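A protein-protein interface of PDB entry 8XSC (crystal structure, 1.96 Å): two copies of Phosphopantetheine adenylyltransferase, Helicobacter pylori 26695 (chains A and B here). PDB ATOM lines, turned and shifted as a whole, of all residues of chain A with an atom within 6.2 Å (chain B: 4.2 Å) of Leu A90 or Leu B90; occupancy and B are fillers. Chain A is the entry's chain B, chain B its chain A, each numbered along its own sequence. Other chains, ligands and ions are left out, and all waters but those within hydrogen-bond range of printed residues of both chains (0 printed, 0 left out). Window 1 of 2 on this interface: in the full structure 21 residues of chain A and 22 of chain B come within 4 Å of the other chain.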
ATOM      1  N   ILE A  21     -26.483   3.650  -2.598  1.00  0.00           N
ATOM      2  CA  ILE A  21     -26.723   2.271  -2.094  1.00  0.00           C
ATOM      3  C   ILE A  21     -28.237   2.083  -1.942  1.00  0.00           C
ATOM      4  O   ILE A  21     -28.777   1.032  -2.392  1.00  0.00           O
ATOM      5  CB  ILE A  21     -25.951   2.028  -0.788  1.00  0.00           C
ATOM      6  CG1 ILE A  21     -24.442   2.212  -0.962  1.00  0.00           C
ATOM      7  CG2 ILE A  21     -26.288   0.663  -0.177  1.00  0.00           C
ATOM      8  CD1 ILE A  21     -23.872   1.448  -2.138  1.00  0.00           C
ATOM      9  N   ARG A  88     -25.454  -4.051   2.579  1.00  0.00           N
ATOM     10  CA  ARG A  88     -24.292  -3.316   3.109  1.00  0.00           C
ATOM     11  C   ARG A  88     -23.611  -2.657   1.930  1.00  0.00           C
ATOM     12  O   ARG A  88     -23.758  -3.158   0.795  1.00  0.00           O
ATOM     13  CB  ARG A  88     -23.325  -4.253   3.837  1.00  0.00           C
ATOM     14  CG  ARG A  88     -23.911  -4.991   5.026  1.00  0.00           C
ATOM     15  CD  ARG A  88     -24.046  -4.068   6.212  1.00  0.00           C
ATOM     16  NE  ARG A  88     -22.706  -3.648   6.673  1.00  0.00           N
ATOM     17  CZ  ARG A  88     -22.400  -2.440   7.192  1.00  0.00           C
ATOM     18  NH1 ARG A  88     -23.333  -1.504   7.319  1.00  0.00           N
ATOM     19  NH2 ARG A  88     -21.154  -2.160   7.553  1.00  0.00           N
ATOM     20  N   GLY A  89     -22.896  -1.573   2.206  1.00  0.00           N
ATOM     21  CA  GLY A  89     -22.146  -0.793   1.207  1.00  0.00           C
ATOM     22  C   GLY A  89     -20.662  -1.033   1.371  1.00  0.00           C
ATOM     23  O   GLY A  89     -20.225  -1.203   2.519  1.00  0.00           O
ATOM     24  N   LEU A  90     -19.925  -1.110   0.266  1.00  0.00           N
ATOM     25  CA  LEU A  90     -18.456  -1.349   0.234  1.00  0.00           C
ATOM     26  C   LEU A  90     -17.792  -0.128  -0.405  1.00  0.00           C
ATOM     27  O   LEU A  90     -18.286   0.338  -1.452  1.00  0.00           O
ATOM     28  CB  LEU A  90     -18.147  -2.595  -0.605  1.00  0.00           C
ATOM     29  CG  LEU A  90     -18.230  -3.939   0.111  1.00  0.00           C
ATOM     30  CD1 LEU A  90     -17.478  -4.993  -0.670  1.00  0.00           C
ATOM     31  CD2 LEU A  90     -17.719  -3.869   1.544  1.00  0.00           C
ATOM     32  N   ARG A  91     -16.712   0.366   0.193  1.00  0.00           N
ATOM     33  CA  ARG A  91     -15.984   1.570  -0.289  1.00  0.00           C
ATOM     34  C   ARG A  91     -14.484   1.325  -0.148  1.00  0.00           C
ATOM     35  O   ARG A  91     -14.095   0.333   0.515  1.00  0.00           O
ATOM     36  CB  ARG A  91     -16.337   2.801   0.545  1.00  0.00           C
ATOM     37  CG  ARG A  91     -17.703   3.414   0.266  1.00  0.00           C
ATOM     38  CD  ARG A  91     -18.208   4.082   1.529  1.00  0.00           C
ATOM     39  NE  ARG A  91     -18.058   3.107   2.604  1.00  0.00           N
ATOM     40  CZ  ARG A  91     -17.406   3.273   3.767  1.00  0.00           C
ATOM     41  NH1 ARG A  91     -17.323   2.256   4.607  1.00  0.00           N
ATOM     42  NH2 ARG A  91     -16.856   4.431   4.098  1.00  0.00           N
ATOM     43  N   VAL A  92     -13.678   2.196  -0.757  1.00  0.00           N
ATOM     44  CA  VAL A  92     -12.185   2.065  -0.776  1.00  0.00           C
ATOM     45  C   VAL A  92     -11.681   1.922   0.666  1.00  0.00           C
ATOM     46  O   VAL A  92     -10.759   1.090   0.881  1.00  0.00           O
ATOM     47  CB  VAL A  92     -11.489   3.268  -1.447  1.00  0.00           C
ATOM     48  CG1 VAL A  92      -9.973   3.127  -1.408  1.00  0.00           C
ATOM     49  CG2 VAL A  92     -11.952   3.483  -2.872  1.00  0.00           C
ATOM     50  N   SER A  94     -13.242   0.703   3.338  1.00  0.00           N
ATOM     51  CA  SER A  94     -13.915  -0.390   4.094  1.00  0.00           C
ATOM     52  C   SER A  94     -12.900  -1.301   4.822  1.00  0.00           C
ATOM     53  O   SER A  94     -11.798  -1.579   4.282  1.00  0.00           O
ATOM     54  CB  SER A  94     -14.795  -1.196   3.201  1.00  0.00           C
ATOM     55  OG  SER A  94     -16.006  -0.510   2.903  1.00  0.00           O
ATOM     56  N   PHE A  96     -12.645  -4.709   5.030  1.00  0.00           N
ATOM     57  CA  PHE A  96     -13.354  -5.738   4.213  1.00  0.00           C
ATOM     58  C   PHE A  96     -13.576  -7.003   5.052  1.00  0.00           C
ATOM     59  O   PHE A  96     -14.674  -7.606   4.985  1.00  0.00           O
ATOM     60  CB  PHE A  96     -12.579  -5.999   2.905  1.00  0.00           C
ATOM     61  CG  PHE A  96     -12.514  -4.787   2.017  1.00  0.00           C
ATOM     62  CD1 PHE A  96     -13.656  -4.356   1.349  1.00  0.00           C
ATOM     63  CD2 PHE A  96     -11.347  -4.049   1.891  1.00  0.00           C
ATOM     64  CE1 PHE A  96     -13.625  -3.215   0.555  1.00  0.00           C
ATOM     65  CE2 PHE A  96     -11.317  -2.902   1.105  1.00  0.00           C
ATOM     66  CZ  PHE A  96     -12.452  -2.493   0.440  1.00  0.00           C
ATOM     67  N   GLU A  99     -16.310  -6.553   7.544  1.00  0.00           N
ATOM     68  CA  GLU A  99     -17.603  -6.728   6.824  1.00  0.00           C
ATOM     69  C   GLU A  99     -17.930  -8.212   6.664  1.00  0.00           C
ATOM     70  O   GLU A  99     -19.111  -8.571   6.907  1.00  0.00           O
ATOM     71  CB  GLU A  99     -17.544  -6.061   5.456  1.00  0.00           C
ATOM     72  CG  GLU A  99     -17.452  -4.568   5.565  1.00  0.00           C
ATOM     73  CD  GLU A  99     -18.800  -3.945   5.918  1.00  0.00           C
ATOM     74  OE1 GLU A  99     -19.816  -4.658   5.867  1.00  0.00           O
ATOM     75  OE2 GLU A  99     -18.822  -2.763   6.280  1.00  0.00           O
ATOM     76  N   LEU A 100     -16.954  -9.044   6.243  1.00  0.00           N
ATOM     77  CA  LEU A 100     -17.176 -10.497   6.102  1.00  0.00           C
ATOM     78  C   LEU A 100     -17.508 -11.077   7.470  1.00  0.00           C
ATOM     79  O   LEU A 100     -18.358 -11.954   7.515  1.00  0.00           O
ATOM     80  CB  LEU A 100     -15.938 -11.212   5.560  1.00  0.00           C
ATOM     81  CG  LEU A 100     -15.563 -10.981   4.106  1.00  0.00           C
ATOM     82  CD1 LEU A 100     -14.418 -11.915   3.758  1.00  0.00           C
ATOM     83  CD2 LEU A 100     -16.748 -11.213   3.172  1.00  0.00           C
ATOM     84  N   TYR A 104     -21.024 -13.317   8.454  1.00  0.00           N
ATOM     85  CA  TYR A 104     -21.044 -14.651   9.095  1.00  0.00           C
ATOM     86  C   TYR A 104     -21.614 -14.600  10.528  1.00  0.00           C
ATOM     87  O   TYR A 104     -22.318 -15.536  10.885  1.00  0.00           O
ATOM     88  CB  TYR A 104     -19.649 -15.256   8.988  1.00  0.00           C
ATOM     89  CG  TYR A 104     -19.245 -15.514   7.557  1.00  0.00           C
ATOM     90  CD1 TYR A 104     -20.113 -16.135   6.661  1.00  0.00           C
ATOM     91  CD2 TYR A 104     -17.991 -15.168   7.099  1.00  0.00           C
ATOM     92  CE1 TYR A 104     -19.744 -16.378   5.348  1.00  0.00           C
ATOM     93  CE2 TYR A 104     -17.588 -15.443   5.798  1.00  0.00           C
ATOM     94  CZ  TYR A 104     -18.482 -16.028   4.911  1.00  0.00           C
ATOM     95  OH  TYR A 104     -18.132 -16.317   3.628  1.00  0.00           O
ATOM     96  N   TYR A 117     -23.496  -6.968  -0.865  1.00  0.00           N
ATOM     97  CA  TYR A 117     -22.689  -5.721  -0.859  1.00  0.00           C
ATOM     98  C   TYR A 117     -22.897  -4.955  -2.159  1.00  0.00           C
ATOM     99  O   TYR A 117     -22.646  -5.532  -3.256  1.00  0.00           O
ATOM    100  CB  TYR A 117     -21.205  -6.022  -0.656  1.00  0.00           C
ATOM    101  CG  TYR A 117     -20.941  -6.730   0.630  1.00  0.00           C
ATOM    102  CD1 TYR A 117     -20.844  -6.023   1.818  1.00  0.00           C
ATOM    103  CD2 TYR A 117     -20.899  -8.111   0.685  1.00  0.00           C
ATOM    104  CE1 TYR A 117     -20.697  -6.673   3.022  1.00  0.00           C
ATOM    105  CE2 TYR A 117     -20.755  -8.781   1.885  1.00  0.00           C
ATOM    106  CZ  TYR A 117     -20.640  -8.050   3.053  1.00  0.00           C
ATOM    107  OH  TYR A 117     -20.469  -8.709   4.228  1.00  0.00           O
ATOM    108  N   PHE A 118     -23.254  -3.681  -2.023  1.00  0.00           N
ATOM    109  CA  PHE A 118     -23.366  -2.703  -3.134  1.00  0.00           C
ATOM    110  C   PHE A 118     -22.190  -1.720  -3.061  1.00  0.00           C
ATOM    111  O   PHE A 118     -21.510  -1.584  -1.990  1.00  0.00           O
ATOM    112  CB  PHE A 118     -24.732  -2.009  -3.125  1.00  0.00           C
ATOM    113  CG  PHE A 118     -25.916  -2.912  -3.350  1.00  0.00           C
ATOM    114  CD1 PHE A 118     -26.352  -3.774  -2.348  1.00  0.00           C
ATOM    115  CD2 PHE A 118     -26.627  -2.879  -4.543  1.00  0.00           C
ATOM    116  CE1 PHE A 118     -27.460  -4.586  -2.533  1.00  0.00           C
ATOM    117  CE2 PHE A 118     -27.722  -3.706  -4.731  1.00  0.00           C
ATOM    118  CZ  PHE A 118     -28.130  -4.562  -3.730  1.00  0.00           C
ATOM    119  N   MET A 119     -21.858  -1.145  -4.210  1.00  0.00           N
ATOM    120  CA  MET A 119     -20.811  -0.082  -4.336  1.00  0.00           C
ATOM    121  C   MET A 119     -21.536   1.221  -4.582  1.00  0.00           C
ATOM    122  O   MET A 119     -22.556   1.212  -5.266  1.00  0.00           O
ATOM    123  CB  MET A 119     -19.879  -0.265  -5.535  1.00  0.00           C
ATOM    124  CG  MET A 119     -19.161  -1.572  -5.588  1.00  0.00           C
ATOM    125  SD  MET A 119     -18.576  -1.881  -7.280  1.00  0.00           S
ATOM    126  CE  MET A 119     -17.600  -0.421  -7.617  1.00  0.00           C
ATOM    127  N   PRO A 120     -21.008   2.363  -4.084  1.00  0.00           N
ATOM    128  CA  PRO A 120     -21.491   3.677  -4.499  1.00  0.00           C
ATOM    129  C   PRO A 120     -20.899   3.946  -5.895  1.00  0.00           C
ATOM    130  O   PRO A 120     -20.015   3.199  -6.347  1.00  0.00           O
ATOM    131  CB  PRO A 120     -20.962   4.609  -3.390  1.00  0.00           C
ATOM    132  CG  PRO A 120     -19.649   3.930  -2.969  1.00  0.00           C
ATOM    133  CD  PRO A 120     -19.894   2.446  -3.138  1.00  0.00           C
ATOM    134  N   ALA A 125     -16.764   7.062  -4.171  1.00  0.00           N
ATOM    135  CA  ALA A 125     -16.110   5.802  -3.724  1.00  0.00           C
ATOM    136  C   ALA A 125     -15.198   6.085  -2.529  1.00  0.00           C
ATOM    137  O   ALA A 125     -14.952   5.153  -1.698  1.00  0.00           O
ATOM    138  CB  ALA A 125     -15.365   5.173  -4.877  1.00  0.00           C
ATOM    139  N   GLY B  89     -18.136 -12.700  -6.214  1.00  0.00           N
ATOM    140  CA  GLY B  89     -18.036 -13.300  -4.876  1.00  0.00           C
ATOM    141  C   GLY B  89     -16.967 -12.610  -4.062  1.00  0.00           C
ATOM    142  O   GLY B  89     -15.955 -12.214  -4.672  1.00  0.00           O
ATOM    143  N   LEU B  90     -17.162 -12.495  -2.746  1.00  0.00           N
ATOM    144  CA  LEU B  90     -16.121 -11.969  -1.821  1.00  0.00           C
ATOM    145  C   LEU B  90     -15.731 -13.061  -0.806  1.00  0.00           C
ATOM    146  O   LEU B  90     -16.637 -13.621  -0.127  1.00  0.00           O
ATOM    147  CB  LEU B  90     -16.618 -10.703  -1.118  1.00  0.00           C
ATOM    148  CG  LEU B  90     -16.745  -9.469  -2.008  1.00  0.00           C
ATOM    149  CD1 LEU B  90     -17.236  -8.280  -1.209  1.00  0.00           C
ATOM    150  CD2 LEU B  90     -15.435  -9.145  -2.725  1.00  0.00           C
ATOM    151  N   ARG B  91     -14.409 -13.267  -0.676  1.00  0.00           N
ATOM    152  CA  ARG B  91     -13.748 -14.329   0.119  1.00  0.00           C
ATOM    153  C   ARG B  91     -12.659 -13.702   0.985  1.00  0.00           C
ATOM    154  O   ARG B  91     -12.239 -12.567   0.715  1.00  0.00           O
ATOM    155  CB  ARG B  91     -13.052 -15.345  -0.776  1.00  0.00           C
ATOM    156  CG  ARG B  91     -13.963 -16.393  -1.395  1.00  0.00           C
ATOM    157  CD  ARG B  91     -13.363 -16.991  -2.653  1.00  0.00           C
ATOM    158  NE  ARG B  91     -12.664 -15.967  -3.420  1.00  0.00           N
ATOM    159  CZ  ARG B  91     -11.389 -16.020  -3.816  1.00  0.00           C
ATOM    160  NH1 ARG B  91     -10.859 -15.011  -4.490  1.00  0.00           N
ATOM    161  NH2 ARG B  91     -10.645 -17.090  -3.582  1.00  0.00           N
ATOM    162  N   SER B  94      -9.856 -12.440  -1.097  1.00  0.00           N
ATOM    163  CA  SER B  94     -10.161 -11.503  -2.214  1.00  0.00           C
ATOM    164  C   SER B  94      -9.175 -10.324  -2.142  1.00  0.00           C
ATOM    165  O   SER B  94      -8.878  -9.834  -1.018  1.00  0.00           O
ATOM    166  CB  SER B  94     -11.590 -10.997  -2.222  1.00  0.00           C
ATOM    167  OG  SER B  94     -12.518 -12.052  -2.367  1.00  0.00           O
ATOM    168  N   PHE B  96      -9.590  -6.974  -2.345  1.00  0.00           N
ATOM    169  CA  PHE B  96     -10.841  -6.188  -2.252  1.00  0.00           C
ATOM    170  C   PHE B  96     -10.715  -4.943  -3.134  1.00  0.00           C
ATOM    171  O   PHE B  96     -11.692  -4.621  -3.815  1.00  0.00           O
ATOM    172  CB  PHE B  96     -11.136  -5.905  -0.785  1.00  0.00           C
ATOM    173  CG  PHE B  96     -11.381  -7.151   0.021  1.00  0.00           C
ATOM    174  CD1 PHE B  96     -12.580  -7.845  -0.076  1.00  0.00           C
ATOM    175  CD2 PHE B  96     -10.438  -7.593   0.945  1.00  0.00           C
ATOM    176  CE1 PHE B  96     -12.819  -8.964   0.716  1.00  0.00           C
ATOM    177  CE2 PHE B  96     -10.681  -8.714   1.720  1.00  0.00           C
ATOM    178  CZ  PHE B  96     -11.863  -9.411   1.589  1.00  0.00           C
ATOM    179  N   TYR B 117     -21.922  -7.737  -4.783  1.00  0.00           N
ATOM    180  CA  TYR B 117     -21.080  -8.814  -4.180  1.00  0.00           C
ATOM    181  C   TYR B 117     -21.858  -9.670  -3.186  1.00  0.00           C
ATOM    182  O   TYR B 117     -22.519  -9.157  -2.265  1.00  0.00           O
ATOM    183  CB  TYR B 117     -19.826  -8.286  -3.485  1.00  0.00           C
ATOM    184  CG  TYR B 117     -18.953  -7.435  -4.366  1.00  0.00           C
ATOM    185  CD1 TYR B 117     -17.999  -8.002  -5.188  1.00  0.00           C
ATOM    186  CD2 TYR B 117     -19.169  -6.071  -4.469  1.00  0.00           C
ATOM    187  CE1 TYR B 117     -17.246  -7.230  -6.056  1.00  0.00           C
ATOM    188  CE2 TYR B 117     -18.392  -5.279  -5.296  1.00  0.00           C
ATOM    189  CZ  TYR B 117     -17.413  -5.863  -6.073  1.00  0.00           C
ATOM    190  OH  TYR B 117     -16.658  -5.113  -6.936  1.00  0.00           O
ATOM    191  N   PHE B 118     -21.712 -10.984  -3.368  1.00  0.00           N
ATOM    192  CA  PHE B 118     -22.244 -12.008  -2.457  1.00  0.00           C
ATOM    193  C   PHE B 118     -21.072 -12.649  -1.737  1.00  0.00           C
ATOM    194  O   PHE B 118     -19.878 -12.452  -2.136  1.00  0.00           O
ATOM    195  CB  PHE B 118     -23.045 -13.061  -3.218  1.00  0.00           C
ATOM    196  CG  PHE B 118     -24.285 -12.520  -3.881  1.00  0.00           C
ATOM    197  CD1 PHE B 118     -24.191 -11.756  -5.036  1.00  0.00           C
ATOM    198  CD2 PHE B 118     -25.546 -12.787  -3.375  1.00  0.00           C
ATOM    199  CE1 PHE B 118     -25.324 -11.268  -5.674  1.00  0.00           C
ATOM    200  CE2 PHE B 118     -26.677 -12.291  -4.012  1.00  0.00           C
ATOM    201  CZ  PHE B 118     -26.561 -11.521  -5.144  1.00  0.00           C
ATOM    202  N   MET B 119     -21.422 -13.410  -0.711  1.00  0.00           N
ATOM    203  CA  MET B 119     -20.450 -14.222   0.055  1.00  0.00           C
ATOM    204  C   MET B 119     -20.801 -15.686  -0.116  1.00  0.00           C
ATOM    205  O   MET B 119     -21.978 -16.056  -0.136  1.00  0.00           O
ATOM    206  CB  MET B 119     -20.494 -13.894   1.545  1.00  0.00           C
ATOM    207  CG  MET B 119     -20.259 -12.440   1.838  1.00  0.00           C
ATOM    208  SD  MET B 119     -20.936 -12.065   3.488  1.00  0.00           S
ATOM    209  CE  MET B 119     -19.939 -13.147   4.508  1.00  0.00           C
ATOM    210  N   PRO B 120     -19.782 -16.561  -0.174  1.00  0.00           N
ATOM    211  CA  PRO B 120     -20.008 -17.993  -0.012  1.00  0.00           C
ATOM    212  C   PRO B 120     -20.325 -18.323   1.461  1.00  0.00           C
ATOM    213  O   PRO B 120     -20.290 -17.422   2.324  1.00  0.00           O
ATOM    214  CB  PRO B 120     -18.647 -18.564  -0.444  1.00  0.00           C
ATOM    215  CG  PRO B 120     -17.678 -17.525   0.113  1.00  0.00           C
ATOM    216  CD  PRO B 120     -18.348 -16.221  -0.261  1.00  0.00           C
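The backbone NH (N) of Tyr A117 sits at hydrogen-bond distance from the backbone carbonyl oxygen (O) of Tyr B117 (2.8 Å).
SD of Met A119 sits at hydrogen-bond distance from OH of Tyr B117 (3.8 Å).
The side-chain hydroxyl of Tyr A117 is in hydrogen-bond range of the side-chain sulfur of Met B119 (3.5 Å).
The backbone carbonyl oxygen of Pro B120 sits at hydrogen-bond distance from the side-chain hydroxyl of Tyr A104 (2.8 Å).
The backbone NH of Leu B90 sits at hydrogen-bond distance from the backbone carbonyl oxygen of Phe B118 (2.8 Å).
The backbone NH of Arg B91 lies within hydrogen-bond range of the side-chain hydroxyl of Ser B94 (2.8 Å).
The backbone NH of Leu A90 lies within hydrogen-bond range of the backbone carbonyl oxygen of Phe A118, 2.8 Å away.
OH of Tyr A117 lies within hydrogen-bond range of O of Glu A99 (3.0 Å).
Among the printed residues, pairs that only touch across the chains: Leu A90 with Leu B90 (3.3 Å), Phe A96 with Phe B96 (3.3 Å), Leu A100 with Arg B91 (3.7 Å), Leu A100 with Met B119 (3.6 Å) and Tyr A104 with Met B119 (3.3 Å).
Of chain B, only Leu B90 comes within 4 Å of Leu A90.
Of the printed residues of chain A, Tyr B117 touches Tyr A117 (2.8 Å) and Met A119 (3.8 Å).
Printed residues of chain B within 4 Å of Leu A100: Arg B91 (3.7 Å) and Met B119 (3.6 Å).
Arg A91 touches none of the printed residues of chain B.
Phe B118 touches none of the printed residues of chain A.
The nearest printed residue of chain B that does not touch Leu A90 is Tyr B117 (4.3 Å).
The nearest residue of chain A that does not touch Leu B90 is Leu A100 (4.1 Å).
Hydrophobic or aromatic side chains of chain B within 4 Å of the printed part of chain A: Leu B90, Phe B96, Tyr B117, Met B119 and Pro B120.
Of the 16 printed residues of chain A, 6 touch a printed residue of chain B.
Hydrophobic or aromatic side chains of chain A within 4 Å of the printed part of chain B: Leu A90, Phe A96, Leu A100, Tyr A104, Tyr A117 and Met A119.
Leu A90 touches its own counterpart, Leu B90.
Phe A96 touches its own counterpart, Phe B96.
Tyr A117 touches its own counterpart, Tyr B117.
Tyr A117 touches Met B119, and with the chains exchanged Met A119 touches Tyr B117.
9 positions are printed for both chains.
Of the 9 pairs that touch across the chains among the printed residues, 5 have their exchanged pair printed and touching as well.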
